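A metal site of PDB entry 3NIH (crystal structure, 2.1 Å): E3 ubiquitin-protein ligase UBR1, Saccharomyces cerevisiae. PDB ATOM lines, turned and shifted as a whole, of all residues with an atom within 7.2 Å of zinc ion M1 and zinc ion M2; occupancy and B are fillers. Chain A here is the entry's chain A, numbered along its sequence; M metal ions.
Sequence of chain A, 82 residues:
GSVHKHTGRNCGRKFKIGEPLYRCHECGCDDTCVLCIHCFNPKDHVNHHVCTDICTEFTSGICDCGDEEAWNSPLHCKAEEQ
Zinc ion M2 is bound by the side-chain sulfur (SG) of Cys 39, the side-chain sulfur (SG) of Cys 63, the side-chain sulfur (SG) of Cys 36 and the side-chain sulfur (SG) of Cys 11.
Within 4 Å of zinc ion M2: Cys 11, Cys 36, Cys 39 and Cys 63.
Along chain A the residues within 4 Å of zinc ion M2 span positions 11 to 63.
The nearest printed residue that does not touch zinc ion M2 is Cys 65 (4.2 Å).
SG of Cys 77 is bound to zinc ion M1 (1.9 Å).
The side-chain sulfur (SG) of Cys 39 is bound to zinc ion M1 (2.3 Å).
NE2 of His 6 is bound to zinc ion M1, 2.3 Å away.
Zinc ion M1 is bound by SG of Cys 65, at 2.5 Å.
The backbone NH (N) of Lys 78 lies within hydrogen-bond range of the backbone carbonyl oxygen (O) of Cys 39 (2.9 Å).
ND1 of His 6 lies within hydrogen-bond range of N of Cys 11 (3.3 Å).
The backbone carbonyl oxygen (O) of Arg 9 sits at hydrogen-bond distance from a ring nitrogen (ND1) of His 6 (2.6 Å).
N of Cys 65 sits close to SG of Cys 63.
N of Cys 63 is in hydrogen-bond range of O of Arg 13, at 3.0 Å.
The backbone carbonyl oxygen (O) of Cys 63 is in hydrogen-bond range of the backbone NH (N) of Gly 12, 3.1 Å away.
N of Cys 11 is in hydrogen-bond range of O of Cys 65, at 2.7 Å.
NH2 of Arg 9 sits at hydrogen-bond distance from O of Cys 11, at 3.2 Å.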
ATOM      1  N   HIS A   4     -25.808   0.438  25.656  1.00  0.00           N
ATOM      2  CA  HIS A   4     -26.319  -0.852  25.166  1.00  0.00           C
ATOM      3  C   HIS A   4     -25.679  -1.324  23.860  1.00  0.00           C
ATOM      4  O   HIS A   4     -26.106  -2.336  23.291  1.00  0.00           O
ATOM      5  CB  HIS A   4     -27.827  -0.772  24.998  1.00  0.00           C
ATOM      6  CG  HIS A   4     -28.511   0.048  26.049  1.00  0.00           C
ATOM      7  ND1 HIS A   4     -28.700  -0.399  27.337  1.00  0.00           N
ATOM      8  CD2 HIS A   4     -29.049   1.285  25.992  1.00  0.00           C
ATOM      9  CE1 HIS A   4     -29.334   0.536  28.033  1.00  0.00           C
ATOM     10  NE2 HIS A   4     -29.565   1.561  27.239  1.00  0.00           N
ATOM     11  N   LYS A   5     -24.655  -0.606  23.389  1.00  0.00           N
ATOM     12  CA  LYS A   5     -23.869  -1.029  22.245  1.00  0.00           C
ATOM     13  C   LYS A   5     -23.301  -2.420  22.515  1.00  0.00           C
ATOM     14  O   LYS A   5     -22.902  -2.729  23.634  1.00  0.00           O
ATOM     15  CB  LYS A   5     -22.706  -0.065  21.974  1.00  0.00           C
ATOM     16  CG  LYS A   5     -23.057   1.206  21.232  1.00  0.00           C
ATOM     17  CD  LYS A   5     -22.948   2.432  22.125  1.00  0.00           C
ATOM     18  CE  LYS A   5     -22.791   3.703  21.295  1.00  0.00           C
ATOM     19  NZ  LYS A   5     -22.809   4.940  22.133  1.00  0.00           N
ATOM     20  N   HIS A   6     -23.285  -3.248  21.475  1.00  0.00           N
ATOM     21  CA  HIS A   6     -22.680  -4.574  21.569  1.00  0.00           C
ATOM     22  C   HIS A   6     -21.952  -4.843  20.256  1.00  0.00           C
ATOM     23  O   HIS A   6     -22.003  -5.955  19.703  1.00  0.00           O
ATOM     24  CB  HIS A   6     -23.747  -5.627  21.861  1.00  0.00           C
ATOM     25  CG  HIS A   6     -24.818  -5.702  20.813  1.00  0.00           C
ATOM     26  ND1 HIS A   6     -24.696  -6.512  19.702  1.00  0.00           N
ATOM     27  CD2 HIS A   6     -26.004  -5.077  20.701  1.00  0.00           C
ATOM     28  CE1 HIS A   6     -25.774  -6.375  18.954  1.00  0.00           C
ATOM     29  NE2 HIS A   6     -26.590  -5.519  19.543  1.00  0.00           N
ATOM     30  N   ARG A   9     -20.725  -8.278  18.098  1.00  0.00           N
ATOM     31  CA  ARG A   9     -21.269  -9.508  18.679  1.00  0.00           C
ATOM     32  C   ARG A   9     -22.786  -9.391  18.796  1.00  0.00           C
ATOM     33  O   ARG A   9     -23.366  -8.350  18.489  1.00  0.00           O
ATOM     34  CB  ARG A   9     -20.628  -9.829  20.038  1.00  0.00           C
ATOM     35  CG  ARG A   9     -20.599  -8.670  21.037  1.00  0.00           C
ATOM     36  CD  ARG A   9     -20.518  -9.162  22.479  1.00  0.00           C
ATOM     37  NE  ARG A   9     -21.859  -9.541  22.984  1.00  0.00           N
ATOM     38  CZ  ARG A   9     -22.140  -9.777  24.267  1.00  0.00           C
ATOM     39  NH1 ARG A   9     -21.173  -9.691  25.207  1.00  0.00           N
ATOM     40  NH2 ARG A   9     -23.402 -10.106  24.613  1.00  0.00           N
ATOM     41  N   ASN A  10     -23.428 -10.480  19.207  1.00  0.00           N
ATOM     42  CA  ASN A  10     -24.870 -10.478  19.384  1.00  0.00           C
ATOM     43  C   ASN A  10     -25.227  -9.650  20.627  1.00  0.00           C
ATOM     44  O   ASN A  10     -24.412  -9.493  21.547  1.00  0.00           O
ATOM     45  CB  ASN A  10     -25.366 -11.907  19.563  1.00  0.00           C
ATOM     46  CG  ASN A  10     -24.893 -12.531  20.859  1.00  0.00           C
ATOM     47  OD1 ASN A  10     -23.686 -12.599  21.129  1.00  0.00           O
ATOM     48  ND2 ASN A  10     -25.831 -12.980  21.673  1.00  0.00           N
ATOM     49  N   CYS A  11     -26.454  -9.133  20.654  1.00  0.00           N
ATOM     50  CA  CYS A  11     -26.936  -8.446  21.836  1.00  0.00           C
ATOM     51  C   CYS A  11     -27.130  -9.445  22.963  1.00  0.00           C
ATOM     52  O   CYS A  11     -26.419  -9.397  23.973  1.00  0.00           O
ATOM     53  CB  CYS A  11     -28.244  -7.686  21.551  1.00  0.00           C
ATOM     54  SG  CYS A  11     -28.904  -6.909  23.033  1.00  0.00           S
ATOM     55  N   GLY A  12     -28.075 -10.358  22.793  1.00  0.00           N
ATOM     56  CA  GLY A  12     -28.351 -11.374  23.805  1.00  0.00           C
ATOM     57  C   GLY A  12     -28.976 -10.837  25.091  1.00  0.00           C
ATOM     58  O   GLY A  12     -29.071 -11.558  26.079  1.00  0.00           O
ATOM     59  N   ARG A  13     -29.376  -9.564  25.075  1.00  0.00           N
ATOM     60  CA  ARG A  13     -30.057  -8.956  26.240  1.00  0.00           C
ATOM     61  C   ARG A  13     -31.283  -9.777  26.612  1.00  0.00           C
ATOM     62  O   ARG A  13     -32.169  -9.986  25.786  1.00  0.00           O
ATOM     63  CB  ARG A  13     -30.484  -7.517  25.948  1.00  0.00           C
ATOM     64  CG  ARG A  13     -31.308  -6.841  27.056  1.00  0.00           C
ATOM     65  CD  ARG A  13     -31.609  -5.391  26.716  1.00  0.00           C
ATOM     66  NE  ARG A  13     -30.588  -4.508  27.261  1.00  0.00           N
ATOM     67  CZ  ARG A  13     -30.639  -3.997  28.493  1.00  0.00           C
ATOM     68  NH1 ARG A  13     -31.684  -4.272  29.276  1.00  0.00           N
ATOM     69  NH2 ARG A  13     -29.664  -3.201  28.933  1.00  0.00           N
ATOM     70  N   PHE A  15     -34.805 -10.417  28.130  1.00  0.00           N
ATOM     71  CA  PHE A  15     -36.024  -9.663  28.411  1.00  0.00           C
ATOM     72  C   PHE A  15     -36.515  -9.927  29.832  1.00  0.00           C
ATOM     73  O   PHE A  15     -36.418 -11.045  30.336  1.00  0.00           O
ATOM     74  CB  PHE A  15     -37.140 -10.002  27.414  1.00  0.00           C
ATOM     75  CG  PHE A  15     -36.833  -9.586  26.003  1.00  0.00           C
ATOM     76  CD1 PHE A  15     -37.001  -8.260  25.603  1.00  0.00           C
ATOM     77  CD2 PHE A  15     -36.361 -10.511  25.084  1.00  0.00           C
ATOM     78  CE1 PHE A  15     -36.708  -7.873  24.297  1.00  0.00           C
ATOM     79  CE2 PHE A  15     -36.063 -10.132  23.758  1.00  0.00           C
ATOM     80  CZ  PHE A  15     -36.228  -8.824  23.371  1.00  0.00           C
ATOM     81  N   VAL A  34     -36.368 -11.774  17.614  1.00  0.00           N
ATOM     82  CA  VAL A  34     -36.836 -10.584  18.321  1.00  0.00           C
ATOM     83  C   VAL A  34     -35.705  -9.574  18.593  1.00  0.00           C
ATOM     84  O   VAL A  34     -34.533  -9.937  18.642  1.00  0.00           O
ATOM     85  CB  VAL A  34     -37.524 -10.952  19.680  1.00  0.00           C
ATOM     86  CG1 VAL A  34     -38.166  -9.732  20.322  1.00  0.00           C
ATOM     87  CG2 VAL A  34     -38.590 -12.021  19.504  1.00  0.00           C
ATOM     88  N   LEU A  35     -36.104  -8.320  18.797  1.00  0.00           N
ATOM     89  CA  LEU A  35     -35.198  -7.214  19.112  1.00  0.00           C
ATOM     90  C   LEU A  35     -35.674  -6.525  20.374  1.00  0.00           C
ATOM     91  O   LEU A  35     -36.875  -6.383  20.591  1.00  0.00           O
ATOM     92  CB  LEU A  35     -35.209  -6.192  17.981  1.00  0.00           C
ATOM     93  CG  LEU A  35     -34.632  -6.683  16.639  1.00  0.00           C
ATOM     94  CD1 LEU A  35     -35.049  -5.762  15.510  1.00  0.00           C
ATOM     95  CD2 LEU A  35     -33.119  -6.747  16.758  1.00  0.00           C
ATOM     96  N   CYS A  36     -34.734  -6.100  21.214  1.00  0.00           N
ATOM     97  CA  CYS A  36     -35.083  -5.271  22.362  1.00  0.00           C
ATOM     98  C   CYS A  36     -35.282  -3.820  21.927  1.00  0.00           C
ATOM     99  O   CYS A  36     -34.982  -3.457  20.790  1.00  0.00           O
ATOM    100  CB  CYS A  36     -34.035  -5.362  23.475  1.00  0.00           C
ATOM    101  SG  CYS A  36     -32.420  -4.587  23.132  1.00  0.00           S
ATOM    102  N   ILE A  37     -35.753  -2.995  22.868  1.00  0.00           N
ATOM    103  CA  ILE A  37     -36.041  -1.579  22.604  1.00  0.00           C
ATOM    104  C   ILE A  37     -34.771  -0.753  22.346  1.00  0.00           C
ATOM    105  O   ILE A  37     -34.806   0.244  21.638  1.00  0.00           O
ATOM    106  CB  ILE A  37     -36.937  -0.965  23.735  1.00  0.00           C
ATOM    107  CG1 ILE A  37     -37.562   0.356  23.266  1.00  0.00           C
ATOM    108  CG2 ILE A  37     -36.132  -0.840  25.063  1.00  0.00           C
ATOM    109  CD1 ILE A  37     -38.752   0.838  24.106  1.00  0.00           C
ATOM    110  N   HIS A  38     -33.647  -1.183  22.906  1.00  0.00           N
ATOM    111  CA  HIS A  38     -32.371  -0.494  22.696  1.00  0.00           C
ATOM    112  C   HIS A  38     -31.781  -0.797  21.312  1.00  0.00           C
ATOM    113  O   HIS A  38     -30.924  -0.047  20.827  1.00  0.00           O
ATOM    114  CB  HIS A  38     -31.375  -0.857  23.797  1.00  0.00           C
ATOM    115  CG  HIS A  38     -31.897  -0.636  25.171  1.00  0.00           C
ATOM    116  ND1 HIS A  38     -31.991  -1.653  26.107  1.00  0.00           N
ATOM    117  CD2 HIS A  38     -32.406   0.464  25.767  1.00  0.00           C
ATOM    118  CE1 HIS A  38     -32.504  -1.173  27.219  1.00  0.00           C
ATOM    119  NE2 HIS A  38     -32.771   0.107  27.046  1.00  0.00           N
ATOM    120  N   CYS A  39     -32.231  -1.882  20.700  1.00  0.00           N
ATOM    121  CA  CYS A  39     -31.652  -2.395  19.460  1.00  0.00           C
ATOM    122  C   CYS A  39     -32.539  -2.070  18.246  1.00  0.00           C
ATOM    123  O   CYS A  39     -32.043  -1.734  17.166  1.00  0.00           O
ATOM    124  CB  CYS A  39     -31.400  -3.912  19.579  1.00  0.00           C
ATOM    125  SG  CYS A  39     -30.027  -4.470  20.702  1.00  0.00           S
ATOM    126  N   PHE A  40     -33.859  -2.169  18.431  1.00  0.00           N
ATOM    127  CA  PHE A  40     -34.820  -1.912  17.360  1.00  0.00           C
ATOM    128  C   PHE A  40     -34.707  -0.495  16.799  1.00  0.00           C
ATOM    129  O   PHE A  40     -34.826   0.507  17.528  1.00  0.00           O
ATOM    130  CB  PHE A  40     -36.256  -2.197  17.828  1.00  0.00           C
ATOM    131  CG  PHE A  40     -37.318  -1.902  16.773  1.00  0.00           C
ATOM    132  CD1 PHE A  40     -37.673  -2.864  15.830  1.00  0.00           C
ATOM    133  CD2 PHE A  40     -37.960  -0.673  16.754  1.00  0.00           C
ATOM    134  CE1 PHE A  40     -38.660  -2.587  14.873  1.00  0.00           C
ATOM    135  CE2 PHE A  40     -38.943  -0.378  15.791  1.00  0.00           C
ATOM    136  CZ  PHE A  40     -39.284  -1.343  14.848  1.00  0.00           C
ATOM    137  N   ILE A  62     -34.167 -13.788  24.649  1.00  0.00           N
ATOM    138  CA  ILE A  62     -33.046 -12.880  24.412  1.00  0.00           C
ATOM    139  C   ILE A  62     -33.162 -12.180  23.066  1.00  0.00           C
ATOM    140  O   ILE A  62     -33.719 -12.713  22.118  1.00  0.00           O
ATOM    141  CB  ILE A  62     -31.670 -13.601  24.490  1.00  0.00           C
ATOM    142  CG1 ILE A  62     -31.590 -14.730  23.462  1.00  0.00           C
ATOM    143  CG2 ILE A  62     -31.414 -14.124  25.924  1.00  0.00           C
ATOM    144  CD1 ILE A  62     -30.176 -15.162  23.083  1.00  0.00           C
ATOM    145  N   CYS A  63     -32.600 -10.974  23.008  1.00  0.00           N
ATOM    146  CA  CYS A  63     -32.625 -10.149  21.819  1.00  0.00           C
ATOM    147  C   CYS A  63     -31.651 -10.737  20.794  1.00  0.00           C
ATOM    148  O   CYS A  63     -30.541 -11.138  21.161  1.00  0.00           O
ATOM    149  CB  CYS A  63     -32.228  -8.726  22.172  1.00  0.00           C
ATOM    150  SG  CYS A  63     -31.846  -7.740  20.757  1.00  0.00           S
ATOM    151  N   ASP A  64     -32.089 -10.803  19.538  1.00  0.00           N
ATOM    152  CA  ASP A  64     -31.330 -11.448  18.453  1.00  0.00           C
ATOM    153  C   ASP A  64     -30.507 -10.474  17.593  1.00  0.00           C
ATOM    154  O   ASP A  64     -29.886 -10.884  16.609  1.00  0.00           O
ATOM    155  CB  ASP A  64     -32.245 -12.291  17.559  1.00  0.00           C
ATOM    156  CG  ASP A  64     -32.938 -13.400  18.319  1.00  0.00           C
ATOM    157  OD1 ASP A  64     -32.247 -14.285  18.860  1.00  0.00           O
ATOM    158  OD2 ASP A  64     -34.188 -13.388  18.392  1.00  0.00           O
ATOM    159  N   CYS A  65     -30.505  -9.198  17.982  1.00  0.00           N
ATOM    160  CA  CYS A  65     -29.699  -8.196  17.270  1.00  0.00           C
ATOM    161  C   CYS A  65     -28.232  -8.608  17.199  1.00  0.00           C
ATOM    162  O   CYS A  65     -27.625  -8.964  18.216  1.00  0.00           O
ATOM    163  CB  CYS A  65     -29.805  -6.839  17.944  1.00  0.00           C
ATOM    164  SG  CYS A  65     -29.098  -5.508  16.947  1.00  0.00           S
ATOM    165  N   GLY A  66     -27.675  -8.562  15.987  1.00  0.00           N
ATOM    166  CA  GLY A  66     -26.303  -8.982  15.754  1.00  0.00           C
ATOM    167  C   GLY A  66     -26.138 -10.481  15.526  1.00  0.00           C
ATOM    168  O   GLY A  66     -25.037 -10.951  15.249  1.00  0.00           O
ATOM    169  N   HIS A  76     -29.404  -2.378  11.661  1.00  0.00           N
ATOM    170  CA  HIS A  76     -28.507  -1.339  12.137  1.00  0.00           C
ATOM    171  C   HIS A  76     -28.915  -0.927  13.552  1.00  0.00           C
ATOM    172  O   HIS A  76     -29.774  -0.054  13.717  1.00  0.00           O
ATOM    173  CB  HIS A  76     -28.528  -0.123  11.208  1.00  0.00           C
ATOM    174  CG  HIS A  76     -28.255  -0.458   9.770  1.00  0.00           C
ATOM    175  ND1 HIS A  76     -29.244  -0.810   8.889  1.00  0.00           N
ATOM    176  CD2 HIS A  76     -27.091  -0.494   9.073  1.00  0.00           C
ATOM    177  CE1 HIS A  76     -28.721  -1.048   7.704  1.00  0.00           C
ATOM    178  NE2 HIS A  76     -27.412  -0.853   7.787  1.00  0.00           N
ATOM    179  N   CYS A  77     -28.281  -1.563  14.547  1.00  0.00           N
ATOM    180  CA  CYS A  77     -28.572  -1.378  15.971  1.00  0.00           C
ATOM    181  C   CYS A  77     -28.854   0.091  16.297  1.00  0.00           C
ATOM    182  O   CYS A  77     -28.042   0.969  15.983  1.00  0.00           O
ATOM    183  CB  CYS A  77     -27.385  -1.904  16.822  1.00  0.00           C
ATOM    184  SG  CYS A  77     -27.787  -2.573  18.484  1.00  0.00           S
ATOM    185  N   LYS A  78     -30.005   0.348  16.920  1.00  0.00           N
ATOM    186  CA  LYS A  78     -30.327   1.702  17.400  1.00  0.00           C
ATOM    187  C   LYS A  78     -29.275   2.214  18.393  1.00  0.00           C
ATOM    188  O   LYS A  78     -28.896   3.378  18.344  1.00  0.00           O
ATOM    189  CB  LYS A  78     -31.722   1.771  18.034  1.00  0.00           C
ATOM    190  CG  LYS A  78     -32.226   3.210  18.277  1.00  0.00           C
ATOM    191  CD  LYS A  78     -33.502   3.238  19.109  1.00  0.00           C
ATOM    192  CE  LYS A  78     -34.085   4.643  19.219  1.00  0.00           C
ATOM    193  NZ  LYS A  78     -33.368   5.507  20.208  1.00  0.00           N
ATOM    194  N   ALA A  79     -28.806   1.323  19.274  1.00  0.00           N
ATOM    195  CA  ALA A  79     -27.777   1.661  20.276  1.00  0.00           C
ATOM    196  C   ALA A  79     -26.461   2.125  19.643  1.00  0.00           C
ATOM    197  O   ALA A  79     -25.698   2.855  20.270  1.00  0.00           O
ATOM    198  CB  ALA A  79     -27.531   0.483  21.210  1.00  0.00           C
ATOM    199  N   GLU A  80     -26.220   1.716  18.392  1.00  0.00           N
ATOM    200  CA  GLU A  80     -25.008   2.065  17.659  1.00  0.00           C
ATOM    201  C   GLU A  80     -25.083   3.477  17.051  1.00  0.00           C
ATOM    202  O   GLU A  80     -24.093   3.970  16.487  1.00  0.00           O
ATOM    203  CB  GLU A  80     -24.734   1.023  16.564  1.00  0.00           C
ATOM    204  CG  GLU A  80     -23.270   0.787  16.234  1.00  0.00           C
ATOM    205  CD  GLU A  80     -22.478   0.224  17.406  1.00  0.00           C
ATOM    206  OE1 GLU A  80     -22.831  -0.869  17.906  1.00  0.00           O
ATOM    207  OE2 GLU A  80     -21.492   0.870  17.816  1.00  0.00           O
HETATM  208 ZN    ZN M   1     -28.469  -4.270  19.011  1.00  0.00          ZN
HETATM  209 ZN    ZN M   2     -30.914  -5.953  21.946  1.00  0.00          ZN
